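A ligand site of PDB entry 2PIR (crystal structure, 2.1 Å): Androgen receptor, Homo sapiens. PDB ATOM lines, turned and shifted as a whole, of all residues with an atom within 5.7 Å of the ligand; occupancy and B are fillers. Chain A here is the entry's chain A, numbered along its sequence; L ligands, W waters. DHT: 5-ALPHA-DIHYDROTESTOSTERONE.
The guanidinium group (NH2) of Arg 84 sits at hydrogen-bond distance from the backbone carbonyl oxygen (O) of Phe 96 (2.8 Å).
NE of Arg 84 lies within hydrogen-bond range of O of Tyr 95, 3.1 Å away.
Merely in contact with the ligand: Leu 36 (3.4 Å), Met 77 (3.7 Å), Met 112 (3.7 Å), Leu 33 (3.8 Å), Phe 208 (3.8 Å), Met 81 (3.8 Å), Phe 96 (3.8 Å), Leu 39 (3.9 Å) and Gln 43 (3.95 Å).
Hydrophobic or aromatic side chains within 4 Å of the ligand: Leu 33, Leu 36, Leu 39, Met 77, Met 81, Phe 96, Met 112 and Phe 208.
Within 4 Å of the ligand: Leu 33, Leu 36, Asn 37, Leu 39, Gln 43, Met 77, Met 81, Arg 84, Phe 96, Met 112, Phe 208 and Thr 209.
Water W1 lies within hydrogen-bond range of O of Met 77, O3 of the ligand and NH1 of Arg 84.
The guanidinium group (NH2) of Arg 84 sits at hydrogen-bond distance from an oxygen (O3) of the ligand.
ND2 of Asn 37 is in hydrogen-bond range of O17 of the ligand (3.0 Å).
The side-chain hydroxyl (OG1) of Thr 209 lies within hydrogen-bond range of an oxygen (O17) of the ligand (3.2 Å).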
ATOM      1  N   LEU A  33       2.830  18.409 -26.781  1.00  0.00           N
ATOM      2  CA  LEU A  33       1.861  17.577 -26.090  1.00  0.00           C
ATOM      3  C   LEU A  33       0.595  18.328 -25.714  1.00  0.00           C
ATOM      4  O   LEU A  33      -0.524  17.807 -25.866  1.00  0.00           O
ATOM      5  CB  LEU A  33       2.488  16.944 -24.840  1.00  0.00           C
ATOM      6  CG  LEU A  33       3.125  15.563 -25.041  1.00  0.00           C
ATOM      7  CD1 LEU A  33       2.022  14.530 -25.383  1.00  0.00           C
ATOM      8  CD2 LEU A  33       4.172  15.616 -26.156  1.00  0.00           C
ATOM      9  N   LEU A  36      -1.586  18.477 -28.605  1.00  0.00           N
ATOM     10  CA  LEU A  36      -2.234  17.198 -28.874  1.00  0.00           C
ATOM     11  C   LEU A  36      -3.372  16.997 -27.897  1.00  0.00           C
ATOM     12  O   LEU A  36      -4.409  16.487 -28.280  1.00  0.00           O
ATOM     13  CB  LEU A  36      -1.253  16.045 -28.738  1.00  0.00           C
ATOM     14  CG  LEU A  36      -0.354  15.783 -29.944  1.00  0.00           C
ATOM     15  CD1 LEU A  36       0.763  14.783 -29.588  1.00  0.00           C
ATOM     16  CD2 LEU A  36      -1.211  15.270 -31.105  1.00  0.00           C
ATOM     17  N   ASN A  37      -3.178  17.393 -26.637  1.00  0.00           N
ATOM     18  CA  ASN A  37      -4.216  17.286 -25.612  1.00  0.00           C
ATOM     19  C   ASN A  37      -5.410  18.122 -26.038  1.00  0.00           C
ATOM     20  O   ASN A  37      -6.553  17.681 -25.921  1.00  0.00           O
ATOM     21  CB  ASN A  37      -3.689  17.789 -24.281  1.00  0.00           C
ATOM     22  CG  ASN A  37      -2.778  16.780 -23.596  1.00  0.00           C
ATOM     23  OD1 ASN A  37      -1.993  17.139 -22.712  1.00  0.00           O
ATOM     24  ND2 ASN A  37      -2.903  15.505 -23.987  1.00  0.00           N
ATOM     25  N   LEU A  39      -6.147  19.087 -29.158  1.00  0.00           N
ATOM     26  CA  LEU A  39      -6.670  18.442 -30.348  1.00  0.00           C
ATOM     27  C   LEU A  39      -7.564  17.283 -29.896  1.00  0.00           C
ATOM     28  O   LEU A  39      -8.590  16.985 -30.509  1.00  0.00           O
ATOM     29  CB  LEU A  39      -5.494  17.935 -31.216  1.00  0.00           C
ATOM     30  CG  LEU A  39      -5.874  17.002 -32.379  1.00  0.00           C
ATOM     31  CD1 LEU A  39      -6.804  17.715 -33.350  1.00  0.00           C
ATOM     32  CD2 LEU A  39      -4.624  16.504 -33.098  1.00  0.00           C
ATOM     33  N   GLY A  40      -7.167  16.637 -28.808  1.00  0.00           N
ATOM     34  CA  GLY A  40      -7.983  15.549 -28.305  1.00  0.00           C
ATOM     35  C   GLY A  40      -9.314  16.026 -27.768  1.00  0.00           C
ATOM     36  O   GLY A  40     -10.347  15.425 -28.050  1.00  0.00           O
ATOM     37  N   GLN A  43     -11.441  16.920 -30.736  1.00  0.00           N
ATOM     38  CA  GLN A  43     -11.838  15.689 -31.409  1.00  0.00           C
ATOM     39  C   GLN A  43     -12.962  14.983 -30.645  1.00  0.00           C
ATOM     40  O   GLN A  43     -13.971  14.593 -31.243  1.00  0.00           O
ATOM     41  CB  GLN A  43     -10.655  14.730 -31.534  1.00  0.00           C
ATOM     42  CG  GLN A  43      -9.625  15.148 -32.570  1.00  0.00           C
ATOM     43  CD  GLN A  43     -10.080  14.847 -33.982  1.00  0.00           C
ATOM     44  OE1 GLN A  43      -9.382  15.160 -34.940  1.00  0.00           O
ATOM     45  NE2 GLN A  43     -11.251  14.214 -34.102  1.00  0.00           N
ATOM     46  N   TRP A  73     -12.225   6.174 -27.511  1.00  0.00           N
ATOM     47  CA  TRP A  73     -11.898   7.459 -28.148  1.00  0.00           C
ATOM     48  C   TRP A  73     -10.442   7.444 -28.626  1.00  0.00           C
ATOM     49  O   TRP A  73     -10.084   8.072 -29.638  1.00  0.00           O
ATOM     50  CB  TRP A  73     -12.131   8.632 -27.159  1.00  0.00           C
ATOM     51  CG  TRP A  73     -11.259   8.583 -25.920  1.00  0.00           C
ATOM     52  CD1 TRP A  73     -11.553   7.999 -24.725  1.00  0.00           C
ATOM     53  CD2 TRP A  73      -9.943   9.144 -25.784  1.00  0.00           C
ATOM     54  NE1 TRP A  73     -10.517   8.161 -23.838  1.00  0.00           N
ATOM     55  CE2 TRP A  73      -9.507   8.851 -24.451  1.00  0.00           C
ATOM     56  CE3 TRP A  73      -9.084   9.866 -26.629  1.00  0.00           C
ATOM     57  CZ2 TRP A  73      -8.256   9.250 -23.958  1.00  0.00           C
ATOM     58  CZ3 TRP A  73      -7.833  10.265 -26.137  1.00  0.00           C
ATOM     59  CH2 TRP A  73      -7.441   9.960 -24.803  1.00  0.00           C
ATOM     60  N   MET A  74      -9.589   6.711 -27.914  1.00  0.00           N
ATOM     61  CA  MET A  74      -8.180   6.623 -28.264  1.00  0.00           C
ATOM     62  C   MET A  74      -7.961   5.814 -29.538  1.00  0.00           C
ATOM     63  O   MET A  74      -7.228   6.219 -30.451  1.00  0.00           O
ATOM     64  CB  MET A  74      -7.387   5.955 -27.156  1.00  0.00           C
ATOM     65  CG  MET A  74      -5.926   5.748 -27.511  1.00  0.00           C
ATOM     66  SD  MET A  74      -4.894   7.276 -27.645  1.00  0.00           S
ATOM     67  CE  MET A  74      -4.807   7.528 -25.666  1.00  0.00           C
ATOM     68  N   MET A  77      -9.644   7.657 -32.814  1.00  0.00           N
ATOM     69  CA  MET A  77      -8.874   8.809 -33.294  1.00  0.00           C
ATOM     70  C   MET A  77      -7.591   8.409 -34.022  1.00  0.00           C
ATOM     71  O   MET A  77      -7.210   9.020 -35.007  1.00  0.00           O
ATOM     72  CB  MET A  77      -8.538   9.754 -32.127  1.00  0.00           C
ATOM     73  CG  MET A  77      -9.732  10.460 -31.545  1.00  0.00           C
ATOM     74  SD  MET A  77      -9.333  11.569 -30.160  1.00  0.00           S
ATOM     75  CE  MET A  77     -11.072  11.190 -29.241  1.00  0.00           C
ATOM     76  N   VAL A  78      -6.913   7.395 -33.491  1.00  0.00           N
ATOM     77  CA  VAL A  78      -5.695   6.917 -34.137  1.00  0.00           C
ATOM     78  C   VAL A  78      -5.936   6.283 -35.512  1.00  0.00           C
ATOM     79  O   VAL A  78      -5.192   6.516 -36.460  1.00  0.00           O
ATOM     80  CB  VAL A  78      -4.984   5.851 -33.266  1.00  0.00           C
ATOM     81  CG1 VAL A  78      -3.724   5.333 -33.991  1.00  0.00           C
ATOM     82  CG2 VAL A  78      -4.575   6.479 -31.925  1.00  0.00           C
ATOM     83  N   MET A  81      -6.500   8.986 -37.811  1.00  0.00           N
ATOM     84  CA  MET A  81      -5.275   9.756 -38.024  1.00  0.00           C
ATOM     85  C   MET A  81      -4.339   9.009 -38.986  1.00  0.00           C
ATOM     86  O   MET A  81      -3.667   9.604 -39.808  1.00  0.00           O
ATOM     87  CB  MET A  81      -4.583  10.004 -36.680  1.00  0.00           C
ATOM     88  CG  MET A  81      -3.262  10.789 -36.744  1.00  0.00           C
ATOM     89  SD  MET A  81      -1.826   9.896 -37.413  1.00  0.00           S
ATOM     90  CE  MET A  81      -1.306   8.942 -36.025  1.00  0.00           C
ATOM     91  N   ARG A  84      -5.669   9.551 -42.544  1.00  0.00           N
ATOM     92  CA  ARG A  84      -5.357  10.895 -43.039  1.00  0.00           C
ATOM     93  C   ARG A  84      -3.891  10.947 -43.481  1.00  0.00           C
ATOM     94  O   ARG A  84      -3.575  11.591 -44.476  1.00  0.00           O
ATOM     95  CB  ARG A  84      -5.592  11.949 -41.948  1.00  0.00           C
ATOM     96  CG  ARG A  84      -7.038  12.073 -41.512  1.00  0.00           C
ATOM     97  CD  ARG A  84      -7.249  13.405 -40.751  1.00  0.00           C
ATOM     98  NE  ARG A  84      -6.490  13.476 -39.496  1.00  0.00           N
ATOM     99  CZ  ARG A  84      -6.963  13.069 -38.322  1.00  0.00           C
ATOM    100  NH1 ARG A  84      -8.198  12.574 -38.233  1.00  0.00           N
ATOM    101  NH2 ARG A  84      -6.210  13.135 -37.230  1.00  0.00           N
ATOM    102  N   TYR A  95      -0.253  12.758 -39.845  1.00  0.00           N
ATOM    103  CA  TYR A  95      -1.121  13.901 -40.088  1.00  0.00           C
ATOM    104  C   TYR A  95      -2.190  14.038 -38.993  1.00  0.00           C
ATOM    105  O   TYR A  95      -3.401  13.822 -39.205  1.00  0.00           O
ATOM    106  CB  TYR A  95      -1.760  13.741 -41.467  1.00  0.00           C
ATOM    107  CG  TYR A  95      -2.300  15.019 -42.066  1.00  0.00           C
ATOM    108  CD1 TYR A  95      -3.498  15.568 -41.645  1.00  0.00           C
ATOM    109  CD2 TYR A  95      -1.583  15.678 -43.065  1.00  0.00           C
ATOM    110  CE1 TYR A  95      -3.976  16.760 -42.206  1.00  0.00           C
ATOM    111  CE2 TYR A  95      -2.046  16.864 -43.630  1.00  0.00           C
ATOM    112  CZ  TYR A  95      -3.236  17.401 -43.209  1.00  0.00           C
ATOM    113  OH  TYR A  95      -3.689  18.568 -43.781  1.00  0.00           O
ATOM    114  N   PHE A  96      -1.732  14.383 -37.795  1.00  0.00           N
ATOM    115  CA  PHE A  96      -2.660  14.582 -36.665  1.00  0.00           C
ATOM    116  C   PHE A  96      -3.705  15.673 -36.980  1.00  0.00           C
ATOM    117  O   PHE A  96      -4.914  15.538 -36.749  1.00  0.00           O
ATOM    118  CB  PHE A  96      -1.891  14.984 -35.408  1.00  0.00           C
ATOM    119  CG  PHE A  96      -1.045  13.887 -34.828  1.00  0.00           C
ATOM    120  CD1 PHE A  96      -1.624  12.694 -34.443  1.00  0.00           C
ATOM    121  CD2 PHE A  96       0.332  14.071 -34.638  1.00  0.00           C
ATOM    122  CE1 PHE A  96      -0.855  11.690 -33.867  1.00  0.00           C
ATOM    123  CE2 PHE A  96       1.121  13.080 -34.055  1.00  0.00           C
ATOM    124  CZ  PHE A  96       0.520  11.881 -33.669  1.00  0.00           C
ATOM    125  N   MET A 112       7.750  10.233 -27.491  1.00  0.00           N
ATOM    126  CA  MET A 112       6.967   9.025 -27.727  1.00  0.00           C
ATOM    127  C   MET A 112       7.222   8.530 -29.139  1.00  0.00           C
ATOM    128  O   MET A 112       6.285   8.222 -29.883  1.00  0.00           O
ATOM    129  CB  MET A 112       5.482   9.292 -27.536  1.00  0.00           C
ATOM    130  CG  MET A 112       4.951  10.447 -28.360  1.00  0.00           C
ATOM    131  SD  MET A 112       3.089  10.491 -28.338  1.00  0.00           S
ATOM    132  CE  MET A 112       2.791  11.944 -27.419  1.00  0.00           C
ATOM    133  N   MET A 119       2.220   3.881 -35.210  1.00  0.00           N
ATOM    134  CA  MET A 119       1.067   4.512 -35.854  1.00  0.00           C
ATOM    135  C   MET A 119       1.355   4.723 -37.337  1.00  0.00           C
ATOM    136  O   MET A 119       0.441   4.661 -38.177  1.00  0.00           O
ATOM    137  CB  MET A 119       0.753   5.859 -35.186  1.00  0.00           C
ATOM    138  CG  MET A 119       0.310   5.739 -33.743  1.00  0.00           C
ATOM    139  SD  MET A 119      -0.343   7.266 -33.071  1.00  0.00           S
ATOM    140  CE  MET A 119       1.235   7.983 -32.376  1.00  0.00           C
ATOM    141  N   LEU A 205      -0.528   4.046 -25.901  1.00  0.00           N
ATOM    142  CA  LEU A 205      -0.814   5.468 -25.777  1.00  0.00           C
ATOM    143  C   LEU A 205      -1.586   5.748 -24.493  1.00  0.00           C
ATOM    144  O   LEU A 205      -1.452   6.817 -23.902  1.00  0.00           O
ATOM    145  CB  LEU A 205      -1.609   5.937 -26.986  1.00  0.00           C
ATOM    146  CG  LEU A 205      -0.888   5.836 -28.345  1.00  0.00           C
ATOM    147  CD1 LEU A 205      -1.830   6.189 -29.454  1.00  0.00           C
ATOM    148  CD2 LEU A 205       0.318   6.748 -28.356  1.00  0.00           C
ATOM    149  N   PHE A 208       0.856   6.065 -21.811  1.00  0.00           N
ATOM    150  CA  PHE A 208       1.653   7.271 -21.979  1.00  0.00           C
ATOM    151  C   PHE A 208       0.898   8.522 -21.549  1.00  0.00           C
ATOM    152  O   PHE A 208       1.470   9.410 -20.916  1.00  0.00           O
ATOM    153  CB  PHE A 208       2.110   7.374 -23.445  1.00  0.00           C
ATOM    154  CG  PHE A 208       3.093   8.475 -23.700  1.00  0.00           C
ATOM    155  CD1 PHE A 208       2.659   9.777 -23.944  1.00  0.00           C
ATOM    156  CD2 PHE A 208       4.456   8.221 -23.684  1.00  0.00           C
ATOM    157  CE1 PHE A 208       3.558  10.796 -24.163  1.00  0.00           C
ATOM    158  CE2 PHE A 208       5.372   9.234 -23.906  1.00  0.00           C
ATOM    159  CZ  PHE A 208       4.914  10.536 -24.143  1.00  0.00           C
ATOM    160  N   THR A 209      -0.387   8.597 -21.860  1.00  0.00           N
ATOM    161  CA  THR A 209      -1.150   9.791 -21.506  1.00  0.00           C
ATOM    162  C   THR A 209      -1.458   9.788 -20.016  1.00  0.00           C
ATOM    163  O   THR A 209      -1.570  10.844 -19.392  1.00  0.00           O
ATOM    164  CB  THR A 209      -2.465   9.867 -22.314  1.00  0.00           C
ATOM    165  OG1 THR A 209      -3.181  11.058 -21.973  1.00  0.00           O
ATOM    166  CG2 THR A 209      -3.329   8.659 -22.042  1.00  0.00           C
ATOM    167  N   LEU A 212       1.683  10.770 -18.134  1.00  0.00           N
ATOM    168  CA  LEU A 212       1.951  12.181 -18.426  1.00  0.00           C
ATOM    169  C   LEU A 212       1.072  13.103 -17.563  1.00  0.00           C
ATOM    170  O   LEU A 212       1.493  14.169 -17.141  1.00  0.00           O
ATOM    171  CB  LEU A 212       1.716  12.447 -19.927  1.00  0.00           C
ATOM    172  CG  LEU A 212       2.004  13.878 -20.403  1.00  0.00           C
ATOM    173  CD1 LEU A 212       3.424  14.279 -20.076  1.00  0.00           C
ATOM    174  CD2 LEU A 212       1.763  13.985 -21.899  1.00  0.00           C
ATOM    175  N   PHE A 223      -3.592  19.905 -19.527  1.00  0.00           N
ATOM    176  CA  PHE A 223      -4.628  18.918 -19.823  1.00  0.00           C
ATOM    177  C   PHE A 223      -6.004  19.566 -19.731  1.00  0.00           C
ATOM    178  O   PHE A 223      -6.372  20.067 -18.678  1.00  0.00           O
ATOM    179  CB  PHE A 223      -4.554  17.727 -18.867  1.00  0.00           C
ATOM    180  CG  PHE A 223      -3.617  16.651 -19.315  1.00  0.00           C
ATOM    181  CD1 PHE A 223      -2.259  16.712 -19.009  1.00  0.00           C
ATOM    182  CD2 PHE A 223      -4.090  15.573 -20.042  1.00  0.00           C
ATOM    183  CE1 PHE A 223      -1.378  15.708 -19.418  1.00  0.00           C
ATOM    184  CE2 PHE A 223      -3.231  14.547 -20.447  1.00  0.00           C
ATOM    185  CZ  PHE A 223      -1.867  14.620 -20.138  1.00  0.00           C
ATOM    186  N   ILE A 231      -9.034  10.598 -18.495  1.00  0.00           N
ATOM    187  CA  ILE A 231      -7.764   9.906 -18.312  1.00  0.00           C
ATOM    188  C   ILE A 231      -7.483   9.422 -16.891  1.00  0.00           C
ATOM    189  O   ILE A 231      -6.780   8.422 -16.687  1.00  0.00           O
ATOM    190  CB  ILE A 231      -6.597  10.805 -18.775  1.00  0.00           C
ATOM    191  CG1 ILE A 231      -6.676  10.997 -20.301  1.00  0.00           C
ATOM    192  CG2 ILE A 231      -5.256  10.205 -18.354  1.00  0.00           C
ATOM    193  CD1 ILE A 231      -5.855  12.149 -20.811  1.00  0.00           C
HETATM  194  C1  DHT L   1      -5.398  13.371 -30.844  1.00  0.00           C
HETATM  195  C2  DHT L   1      -6.296  13.087 -32.012  1.00  0.00           C
HETATM  196  C3  DHT L   1      -5.444  12.367 -33.090  1.00  0.00           C
HETATM  197  O3  DHT L   1      -5.491  12.712 -34.198  1.00  0.00           O
HETATM  198  C4  DHT L   1      -4.747  11.117 -32.673  1.00  0.00           C
HETATM  199  C5  DHT L   1      -3.822  11.386 -31.496  1.00  0.00           C
HETATM  200  C6  DHT L   1      -3.049  10.119 -30.963  1.00  0.00           C
HETATM  201  C7  DHT L   1      -2.078  10.538 -29.801  1.00  0.00           C
HETATM  202  C8  DHT L   1      -2.785  11.229 -28.587  1.00  0.00           C
HETATM  203  C9  DHT L   1      -3.599  12.459 -29.123  1.00  0.00           C
HETATM  204  C10 DHT L   1      -4.630  12.102 -30.294  1.00  0.00           C
HETATM  205  C11 DHT L   1      -4.288  13.154 -27.892  1.00  0.00           C
HETATM  206  C12 DHT L   1      -3.393  13.530 -26.676  1.00  0.00           C
HETATM  207  C13 DHT L   1      -2.510  12.330 -26.228  1.00  0.00           C
HETATM  208  C14 DHT L   1      -1.815  11.665 -27.459  1.00  0.00           C
HETATM  209  C15 DHT L   1      -0.991  10.570 -26.812  1.00  0.00           C
HETATM  210  C16 DHT L   1      -0.383  11.290 -25.605  1.00  0.00           C
HETATM  211  C17 DHT L   1      -1.227  12.599 -25.431  1.00  0.00           C
HETATM  212  O17 DHT L   1      -1.458  12.862 -24.029  1.00  0.00           O
HETATM  213  C18 DHT L   1      -3.404  11.301 -25.465  1.00  0.00           C
HETATM  214  C19 DHT L   1      -5.700  11.098 -29.687  1.00  0.00           C
HETATM  215  O   HOH W   1      -8.174  11.278 -35.249  1.00  0.00           O
